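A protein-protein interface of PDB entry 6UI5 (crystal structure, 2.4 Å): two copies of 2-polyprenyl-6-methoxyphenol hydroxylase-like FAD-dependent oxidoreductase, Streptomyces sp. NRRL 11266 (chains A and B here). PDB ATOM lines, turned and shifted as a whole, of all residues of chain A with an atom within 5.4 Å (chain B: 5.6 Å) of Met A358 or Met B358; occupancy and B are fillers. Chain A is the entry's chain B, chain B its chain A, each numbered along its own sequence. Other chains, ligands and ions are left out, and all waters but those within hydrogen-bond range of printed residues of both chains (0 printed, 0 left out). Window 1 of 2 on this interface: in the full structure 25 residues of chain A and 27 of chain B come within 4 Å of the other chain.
Gln A343 touches Tyr B357 (NE2 to CE2, 3.5 Å).
CB of Ala A344 touches SD of Met B361 (3.8 Å).
CD1 of Leu B354 touches CD2 of Leu A354, 3.7 Å away.
Met B358 touches Met A358 (CE to CE, 3.6 Å).
Met A361 touches Ala B344 (CE to CB, 3.7 Å).
Met B358 touches just one residue of chain A: Met A358 (3.6 Å).
Of the printed residues of chain B, Ala A344 touches Met B361 (3.8 Å).
Of the printed residues of chain A, Tyr B357 touches Gln A343.
Of the printed residues of chain B, Leu A354 touches Leu B354 (3.7 Å).
Of the printed residues of chain A, Met B361 touches Ala A344 (3.8 Å).
The nearest residue of chain B that does not touch Met A358 is Ala B347 (4.4 Å).
Of the 14 printed residues of chain B, 5 touch a printed residue of chain A.
Printed residues of chain B that touch a printed residue of chain A: Ala B344, Leu B354, Tyr B357, Met B358 and Met B361.
Along chain B the printed residues that touch a printed residue of chain A span positions 344 to 361.
Along chain A the printed residues that touch a printed residue of chain B span positions 343 to 361.
Ala A344 touches Met B361, and with the chains exchanged Met A361 touches Ala B344.
Leu A354 touches its own counterpart, Leu B354.
Met A358 touches its own counterpart, Met B358.
Positions printed for both chains: 344, 347, 348, 354, 355, 356, 357, 358, 359, 360, 361, 362 and 363.
Of the 5 pairs that touch across the chains among the printed residues, 4 have their exchanged pair printed and touching as well.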
ATOM      1  N   GLN A 343      27.507   3.196 -14.438  1.00  0.00           N
ATOM      2  CA  GLN A 343      26.748   3.541 -15.632  1.00  0.00           C
ATOM      3  C   GLN A 343      26.017   2.329 -16.176  1.00  0.00           C
ATOM      4  O   GLN A 343      24.876   2.448 -16.653  1.00  0.00           O
ATOM      5  CB  GLN A 343      27.666   4.138 -16.687  1.00  0.00           C
ATOM      6  CG  GLN A 343      28.178   5.534 -16.315  1.00  0.00           C
ATOM      7  CD  GLN A 343      27.073   6.583 -16.257  1.00  0.00           C
ATOM      8  OE1 GLN A 343      26.178   6.569 -15.388  1.00  0.00           O
ATOM      9  NE2 GLN A 343      27.112   7.490 -17.215  1.00  0.00           N
ATOM     10  N   ALA A 344      26.644   1.144 -16.088  1.00  0.00           N
ATOM     11  CA  ALA A 344      25.961  -0.038 -16.585  1.00  0.00           C
ATOM     12  C   ALA A 344      24.741  -0.340 -15.743  1.00  0.00           C
ATOM     13  O   ALA A 344      23.762  -0.883 -16.265  1.00  0.00           O
ATOM     14  CB  ALA A 344      26.892  -1.253 -16.632  1.00  0.00           C
ATOM     15  N   ALA A 347      21.838   1.924 -16.799  1.00  0.00           N
ATOM     16  CA  ALA A 347      21.270   1.517 -18.074  1.00  0.00           C
ATOM     17  C   ALA A 347      20.174   0.483 -17.906  1.00  0.00           C
ATOM     18  O   ALA A 347      19.425   0.236 -18.864  1.00  0.00           O
ATOM     19  CB  ALA A 347      22.373   0.988 -19.006  1.00  0.00           C
ATOM     20  N   LEU A 348      20.064  -0.144 -16.730  1.00  0.00           N
ATOM     21  CA  LEU A 348      18.951  -1.052 -16.483  1.00  0.00           C
ATOM     22  C   LEU A 348      17.762  -0.346 -15.851  1.00  0.00           C
ATOM     23  O   LEU A 348      16.768  -0.999 -15.520  1.00  0.00           O
ATOM     24  CB  LEU A 348      19.387  -2.251 -15.619  1.00  0.00           C
ATOM     25  CG  LEU A 348      20.454  -3.161 -16.233  1.00  0.00           C
ATOM     26  CD1 LEU A 348      21.764  -2.868 -15.617  1.00  0.00           C
ATOM     27  CD2 LEU A 348      20.148  -4.605 -16.018  1.00  0.00           C
ATOM     28  N   LEU A 354      15.706   1.385 -23.276  1.00  0.00           N
ATOM     29  CA  LEU A 354      17.020   0.776 -23.126  1.00  0.00           C
ATOM     30  C   LEU A 354      17.049  -0.197 -21.950  1.00  0.00           C
ATOM     31  O   LEU A 354      17.571  -1.306 -22.070  1.00  0.00           O
ATOM     32  CB  LEU A 354      18.084   1.857 -22.953  1.00  0.00           C
ATOM     33  CG  LEU A 354      19.409   1.358 -22.394  1.00  0.00           C
ATOM     34  CD1 LEU A 354      20.223   0.678 -23.483  1.00  0.00           C
ATOM     35  CD2 LEU A 354      20.157   2.543 -21.810  1.00  0.00           C
ATOM     36  N   ALA A 355      16.500   0.201 -20.802  1.00  0.00           N
ATOM     37  CA  ALA A 355      16.483  -0.692 -19.642  1.00  0.00           C
ATOM     38  C   ALA A 355      15.866  -2.039 -19.989  1.00  0.00           C
ATOM     39  O   ALA A 355      16.351  -3.085 -19.538  1.00  0.00           O
ATOM     40  CB  ALA A 355      15.724  -0.045 -18.480  1.00  0.00           C
ATOM     41  N   ARG A 356      14.831  -2.042 -20.835  1.00  0.00           N
ATOM     42  CA  ARG A 356      14.105  -3.281 -21.094  1.00  0.00           C
ATOM     43  C   ARG A 356      15.028  -4.360 -21.647  1.00  0.00           C
ATOM     44  O   ARG A 356      14.982  -5.517 -21.209  1.00  0.00           O
ATOM     45  CB  ARG A 356      12.950  -3.037 -22.054  1.00  0.00           C
ATOM     46  CG  ARG A 356      12.463  -4.322 -22.676  1.00  0.00           C
ATOM     47  CD  ARG A 356      11.899  -4.069 -24.051  1.00  0.00           C
ATOM     48  NE  ARG A 356      10.609  -3.392 -23.990  1.00  0.00           N
ATOM     49  CZ  ARG A 356       9.435  -4.015 -23.974  1.00  0.00           C
ATOM     50  NH1 ARG A 356       9.381  -5.342 -24.005  1.00  0.00           N
ATOM     51  NH2 ARG A 356       8.314  -3.305 -23.936  1.00  0.00           N
ATOM     52  N   TYR A 357      15.876  -3.998 -22.616  1.00  0.00           N
ATOM     53  CA  TYR A 357      16.741  -4.990 -23.242  1.00  0.00           C
ATOM     54  C   TYR A 357      18.024  -5.213 -22.452  1.00  0.00           C
ATOM     55  O   TYR A 357      18.548  -6.330 -22.444  1.00  0.00           O
ATOM     56  CB  TYR A 357      17.053  -4.578 -24.681  1.00  0.00           C
ATOM     57  CG  TYR A 357      15.813  -4.500 -25.546  1.00  0.00           C
ATOM     58  CD1 TYR A 357      15.179  -5.660 -25.983  1.00  0.00           C
ATOM     59  CD2 TYR A 357      15.272  -3.277 -25.903  1.00  0.00           C
ATOM     60  CE1 TYR A 357      14.052  -5.612 -26.757  1.00  0.00           C
ATOM     61  CE2 TYR A 357      14.135  -3.207 -26.679  1.00  0.00           C
ATOM     62  CZ  TYR A 357      13.526  -4.371 -27.102  1.00  0.00           C
ATOM     63  OH  TYR A 357      12.388  -4.288 -27.869  1.00  0.00           O
ATOM     64  N   MET A 358      18.556  -4.184 -21.793  1.00  0.00           N
ATOM     65  CA  MET A 358      19.749  -4.408 -20.985  1.00  0.00           C
ATOM     66  C   MET A 358      19.446  -5.330 -19.820  1.00  0.00           C
ATOM     67  O   MET A 358      20.292  -6.143 -19.433  1.00  0.00           O
ATOM     68  CB  MET A 358      20.317  -3.092 -20.452  1.00  0.00           C
ATOM     69  CG  MET A 358      20.740  -2.098 -21.515  1.00  0.00           C
ATOM     70  SD  MET A 358      21.960  -2.793 -22.632  1.00  0.00           S
ATOM     71  CE  MET A 358      23.064  -3.602 -21.455  1.00  0.00           C
ATOM     72  N   ARG A 359      18.251  -5.208 -19.242  1.00  0.00           N
ATOM     73  CA  ARG A 359      17.896  -6.073 -18.124  1.00  0.00           C
ATOM     74  C   ARG A 359      17.928  -7.532 -18.553  1.00  0.00           C
ATOM     75  O   ARG A 359      18.649  -8.345 -17.957  1.00  0.00           O
ATOM     76  CB  ARG A 359      16.533  -5.670 -17.542  1.00  0.00           C
ATOM     77  CG  ARG A 359      16.597  -4.348 -16.764  1.00  0.00           C
ATOM     78  CD  ARG A 359      15.218  -3.834 -16.322  1.00  0.00           C
ATOM     79  NE  ARG A 359      14.741  -4.485 -15.100  1.00  0.00           N
ATOM     80  CZ  ARG A 359      15.231  -4.270 -13.874  1.00  0.00           C
ATOM     81  NH1 ARG A 359      16.237  -3.419 -13.675  1.00  0.00           N
ATOM     82  NH2 ARG A 359      14.716  -4.921 -12.837  1.00  0.00           N
ATOM     83  N   GLU A 360      17.206  -7.864 -19.630  1.00  0.00           N
ATOM     84  CA  GLU A 360      17.288  -9.208 -20.201  1.00  0.00           C
ATOM     85  C   GLU A 360      18.731  -9.602 -20.478  1.00  0.00           C
ATOM     86  O   GLU A 360      19.159 -10.715 -20.141  1.00  0.00           O
ATOM     87  CB  GLU A 360      16.461  -9.296 -21.487  1.00  0.00           C
ATOM     88  CG  GLU A 360      14.990  -9.013 -21.301  1.00  0.00           C
ATOM     89  CD  GLU A 360      14.196  -9.186 -22.591  1.00  0.00           C
ATOM     90  OE1 GLU A 360      14.812  -9.519 -23.627  1.00  0.00           O
ATOM     91  OE2 GLU A 360      12.955  -8.997 -22.570  1.00  0.00           O
ATOM     92  N   MET A 361      19.499  -8.685 -21.081  1.00  0.00           N
ATOM     93  CA  MET A 361      20.905  -8.964 -21.353  1.00  0.00           C
ATOM     94  C   MET A 361      21.630  -9.371 -20.082  1.00  0.00           C
ATOM     95  O   MET A 361      22.365 -10.356 -20.074  1.00  0.00           O
ATOM     96  CB  MET A 361      21.589  -7.755 -21.981  1.00  0.00           C
ATOM     97  CG  MET A 361      22.866  -8.136 -22.682  1.00  0.00           C
ATOM     98  SD  MET A 361      22.488  -9.335 -23.995  1.00  0.00           S
ATOM     99  CE  MET A 361      24.047  -9.334 -24.841  1.00  0.00           C
ATOM    100  N   MET A 362      21.438  -8.611 -19.005  1.00  0.00           N
ATOM    101  CA  MET A 362      22.152  -8.897 -17.779  1.00  0.00           C
ATOM    102  C   MET A 362      21.636 -10.184 -17.158  1.00  0.00           C
ATOM    103  O   MET A 362      22.422 -10.981 -16.626  1.00  0.00           O
ATOM    104  CB  MET A 362      22.030  -7.717 -16.812  1.00  0.00           C
ATOM    105  CG  MET A 362      23.080  -6.653 -17.007  1.00  0.00           C
ATOM    106  SD  MET A 362      24.775  -7.289 -17.083  1.00  0.00           S
ATOM    107  CE  MET A 362      25.028  -7.799 -15.397  1.00  0.00           C
ATOM    108  N   GLY A 363      20.317 -10.407 -17.241  1.00  0.00           N
ATOM    109  CA  GLY A 363      19.768 -11.706 -16.892  1.00  0.00           C
ATOM    110  C   GLY A 363      20.553 -12.841 -17.516  1.00  0.00           C
ATOM    111  O   GLY A 363      20.858 -13.834 -16.857  1.00  0.00           O
ATOM    112  N   ALA B 344      21.346  -4.872 -27.731  1.00  0.00           N
ATOM    113  CA  ALA B 344      22.575  -4.741 -26.955  1.00  0.00           C
ATOM    114  C   ALA B 344      23.734  -4.322 -27.842  1.00  0.00           C
ATOM    115  O   ALA B 344      24.539  -3.478 -27.450  1.00  0.00           O
ATOM    116  CB  ALA B 344      22.920  -6.051 -26.230  1.00  0.00           C
ATOM    117  N   ALA B 347      23.588  -0.632 -28.431  1.00  0.00           N
ATOM    118  CA  ALA B 347      23.921   0.245 -27.310  1.00  0.00           C
ATOM    119  C   ALA B 347      25.414   0.451 -27.154  1.00  0.00           C
ATOM    120  O   ALA B 347      25.815   1.196 -26.256  1.00  0.00           O
ATOM    121  CB  ALA B 347      23.338  -0.301 -26.007  1.00  0.00           C
ATOM    122  N   LEU B 348      26.240  -0.195 -27.979  1.00  0.00           N
ATOM    123  CA  LEU B 348      27.653   0.151 -28.082  1.00  0.00           C
ATOM    124  C   LEU B 348      27.918   1.185 -29.170  1.00  0.00           C
ATOM    125  O   LEU B 348      29.079   1.548 -29.398  1.00  0.00           O
ATOM    126  CB  LEU B 348      28.511  -1.096 -28.341  1.00  0.00           C
ATOM    127  CG  LEU B 348      28.574  -2.148 -27.232  1.00  0.00           C
ATOM    128  CD1 LEU B 348      27.324  -2.954 -27.179  1.00  0.00           C
ATOM    129  CD2 LEU B 348      29.782  -3.069 -27.388  1.00  0.00           C
ATOM    130  N   PRO B 353      27.243   8.849 -25.277  1.00  0.00           N
ATOM    131  CA  PRO B 353      27.492   8.635 -23.829  1.00  0.00           C
ATOM    132  C   PRO B 353      27.283   7.192 -23.363  1.00  0.00           C
ATOM    133  O   PRO B 353      28.120   6.630 -22.629  1.00  0.00           O
ATOM    134  CB  PRO B 353      26.491   9.587 -23.156  1.00  0.00           C
ATOM    135  CG  PRO B 353      25.506   9.972 -24.247  1.00  0.00           C
ATOM    136  CD  PRO B 353      26.299   9.961 -25.501  1.00  0.00           C
ATOM    137  N   LEU B 354      26.150   6.593 -23.736  1.00  0.00           N
ATOM    138  CA  LEU B 354      25.914   5.189 -23.440  1.00  0.00           C
ATOM    139  C   LEU B 354      27.018   4.317 -24.035  1.00  0.00           C
ATOM    140  O   LEU B 354      27.645   3.529 -23.322  1.00  0.00           O
ATOM    141  CB  LEU B 354      24.535   4.780 -23.965  1.00  0.00           C
ATOM    142  CG  LEU B 354      24.075   3.331 -23.742  1.00  0.00           C
ATOM    143  CD1 LEU B 354      23.782   3.028 -22.236  1.00  0.00           C
ATOM    144  CD2 LEU B 354      22.855   3.004 -24.616  1.00  0.00           C
ATOM    145  N   ALA B 355      27.319   4.494 -25.323  1.00  0.00           N
ATOM    146  CA  ALA B 355      28.324   3.650 -25.969  1.00  0.00           C
ATOM    147  C   ALA B 355      29.682   3.748 -25.282  1.00  0.00           C
ATOM    148  O   ALA B 355      30.413   2.752 -25.204  1.00  0.00           O
ATOM    149  CB  ALA B 355      28.460   4.008 -27.446  1.00  0.00           C
ATOM    150  N   ARG B 356      30.041   4.934 -24.780  1.00  0.00           N
ATOM    151  CA  ARG B 356      31.339   5.095 -24.134  1.00  0.00           C
ATOM    152  C   ARG B 356      31.555   4.008 -23.084  1.00  0.00           C
ATOM    153  O   ARG B 356      32.513   3.233 -23.172  1.00  0.00           O
ATOM    154  CB  ARG B 356      31.455   6.490 -23.516  1.00  0.00           C
ATOM    155  CG  ARG B 356      32.588   6.626 -22.522  1.00  0.00           C
ATOM    156  CD  ARG B 356      32.629   8.035 -21.930  1.00  0.00           C
ATOM    157  NE  ARG B 356      33.625   8.923 -22.542  1.00  0.00           N
ATOM    158  CZ  ARG B 356      34.931   8.859 -22.286  1.00  0.00           C
ATOM    159  NH1 ARG B 356      35.405   7.944 -21.445  1.00  0.00           N
ATOM    160  NH2 ARG B 356      35.769   9.700 -22.873  1.00  0.00           N
ATOM    161  N   TYR B 357      30.613   3.879 -22.137  1.00  0.00           N
ATOM    162  CA  TYR B 357      30.788   2.959 -21.015  1.00  0.00           C
ATOM    163  C   TYR B 357      30.367   1.534 -21.363  1.00  0.00           C
ATOM    164  O   TYR B 357      31.018   0.584 -20.909  1.00  0.00           O
ATOM    165  CB  TYR B 357      30.026   3.463 -19.781  1.00  0.00           C
ATOM    166  CG  TYR B 357      30.409   4.871 -19.410  1.00  0.00           C
ATOM    167  CD1 TYR B 357      31.685   5.154 -18.926  1.00  0.00           C
ATOM    168  CD2 TYR B 357      29.517   5.928 -19.583  1.00  0.00           C
ATOM    169  CE1 TYR B 357      32.062   6.447 -18.613  1.00  0.00           C
ATOM    170  CE2 TYR B 357      29.885   7.234 -19.272  1.00  0.00           C
ATOM    171  CZ  TYR B 357      31.162   7.479 -18.789  1.00  0.00           C
ATOM    172  OH  TYR B 357      31.558   8.744 -18.476  1.00  0.00           O
ATOM    173  N   MET B 358      29.289   1.356 -22.156  1.00  0.00           N
ATOM    174  CA  MET B 358      28.876   0.005 -22.542  1.00  0.00           C
ATOM    175  C   MET B 358      29.942  -0.725 -23.352  1.00  0.00           C
ATOM    176  O   MET B 358      29.918  -1.957 -23.396  1.00  0.00           O
ATOM    177  CB  MET B 358      27.576  -0.021 -23.357  1.00  0.00           C
ATOM    178  CG  MET B 358      26.457   0.738 -22.775  1.00  0.00           C
ATOM    179  SD  MET B 358      25.985   0.144 -21.120  1.00  0.00           S
ATOM    180  CE  MET B 358      26.077  -1.647 -21.223  1.00  0.00           C
ATOM    181  N   ARG B 359      30.859   0.002 -23.990  1.00  0.00           N
ATOM    182  CA  ARG B 359      31.950  -0.631 -24.722  1.00  0.00           C
ATOM    183  C   ARG B 359      33.039  -1.095 -23.778  1.00  0.00           C
ATOM    184  O   ARG B 359      33.588  -2.190 -23.949  1.00  0.00           O
ATOM    185  CB  ARG B 359      32.555   0.327 -25.746  1.00  0.00           C
ATOM    186  CG  ARG B 359      31.682   0.605 -26.950  1.00  0.00           C
ATOM    187  CD  ARG B 359      32.392   1.586 -27.868  1.00  0.00           C
ATOM    188  NE  ARG B 359      33.582   0.958 -28.412  1.00  0.00           N
ATOM    189  CZ  ARG B 359      33.587   0.263 -29.541  1.00  0.00           C
ATOM    190  NH1 ARG B 359      32.466   0.137 -30.238  1.00  0.00           N
ATOM    191  NH2 ARG B 359      34.708  -0.304 -29.970  1.00  0.00           N
ATOM    192  N   GLU B 360      33.393  -0.246 -22.813  1.00  0.00           N
ATOM    193  CA  GLU B 360      34.267  -0.691 -21.743  1.00  0.00           C
ATOM    194  C   GLU B 360      33.670  -1.900 -21.030  1.00  0.00           C
ATOM    195  O   GLU B 360      34.376  -2.876 -20.763  1.00  0.00           O
ATOM    196  CB  GLU B 360      34.542   0.471 -20.777  1.00  0.00           C
ATOM    197  CG  GLU B 360      35.523   1.504 -21.373  1.00  0.00           C
ATOM    198  CD  GLU B 360      35.887   2.651 -20.428  1.00  0.00           C
ATOM    199  OE1 GLU B 360      35.505   2.595 -19.240  1.00  0.00           O
ATOM    200  OE2 GLU B 360      36.550   3.617 -20.882  1.00  0.00           O
ATOM    201  N   MET B 361      32.358  -1.872 -20.769  1.00  0.00           N
ATOM    202  CA  MET B 361      31.697  -2.948 -20.033  1.00  0.00           C
ATOM    203  C   MET B 361      31.810  -4.269 -20.787  1.00  0.00           C
ATOM    204  O   MET B 361      32.400  -5.234 -20.284  1.00  0.00           O
ATOM    205  CB  MET B 361      30.231  -2.583 -19.761  1.00  0.00           C
ATOM    206  CG  MET B 361      29.481  -3.524 -18.792  1.00  0.00           C
ATOM    207  SD  MET B 361      29.946  -3.475 -17.006  1.00  0.00           S
ATOM    208  CE  MET B 361      31.334  -4.610 -16.920  1.00  0.00           C
ATOM    209  N   MET B 362      31.273  -4.319 -22.015  1.00  0.00           N
ATOM    210  CA  MET B 362      31.452  -5.489 -22.874  1.00  0.00           C
ATOM    211  C   MET B 362      32.920  -5.841 -23.038  1.00  0.00           C
ATOM    212  O   MET B 362      33.259  -7.024 -23.179  1.00  0.00           O
ATOM    213  CB  MET B 362      30.820  -5.240 -24.250  1.00  0.00           C
ATOM    214  CG  MET B 362      29.327  -5.462 -24.275  1.00  0.00           C
ATOM    215  SD  MET B 362      28.982  -7.172 -23.812  1.00  0.00           S
ATOM    216  CE  MET B 362      29.841  -8.016 -25.133  1.00  0.00           C
ATOM    217  N   GLY B 363      33.803  -4.832 -23.028  1.00  0.00           N
ATOM    218  CA  GLY B 363      35.234  -5.113 -23.019  1.00  0.00           C
ATOM    219  C   GLY B 363      35.622  -6.061 -21.898  1.00  0.00           C
ATOM    220  O   GLY B 363      36.366  -7.019 -22.109  1.00  0.00           O
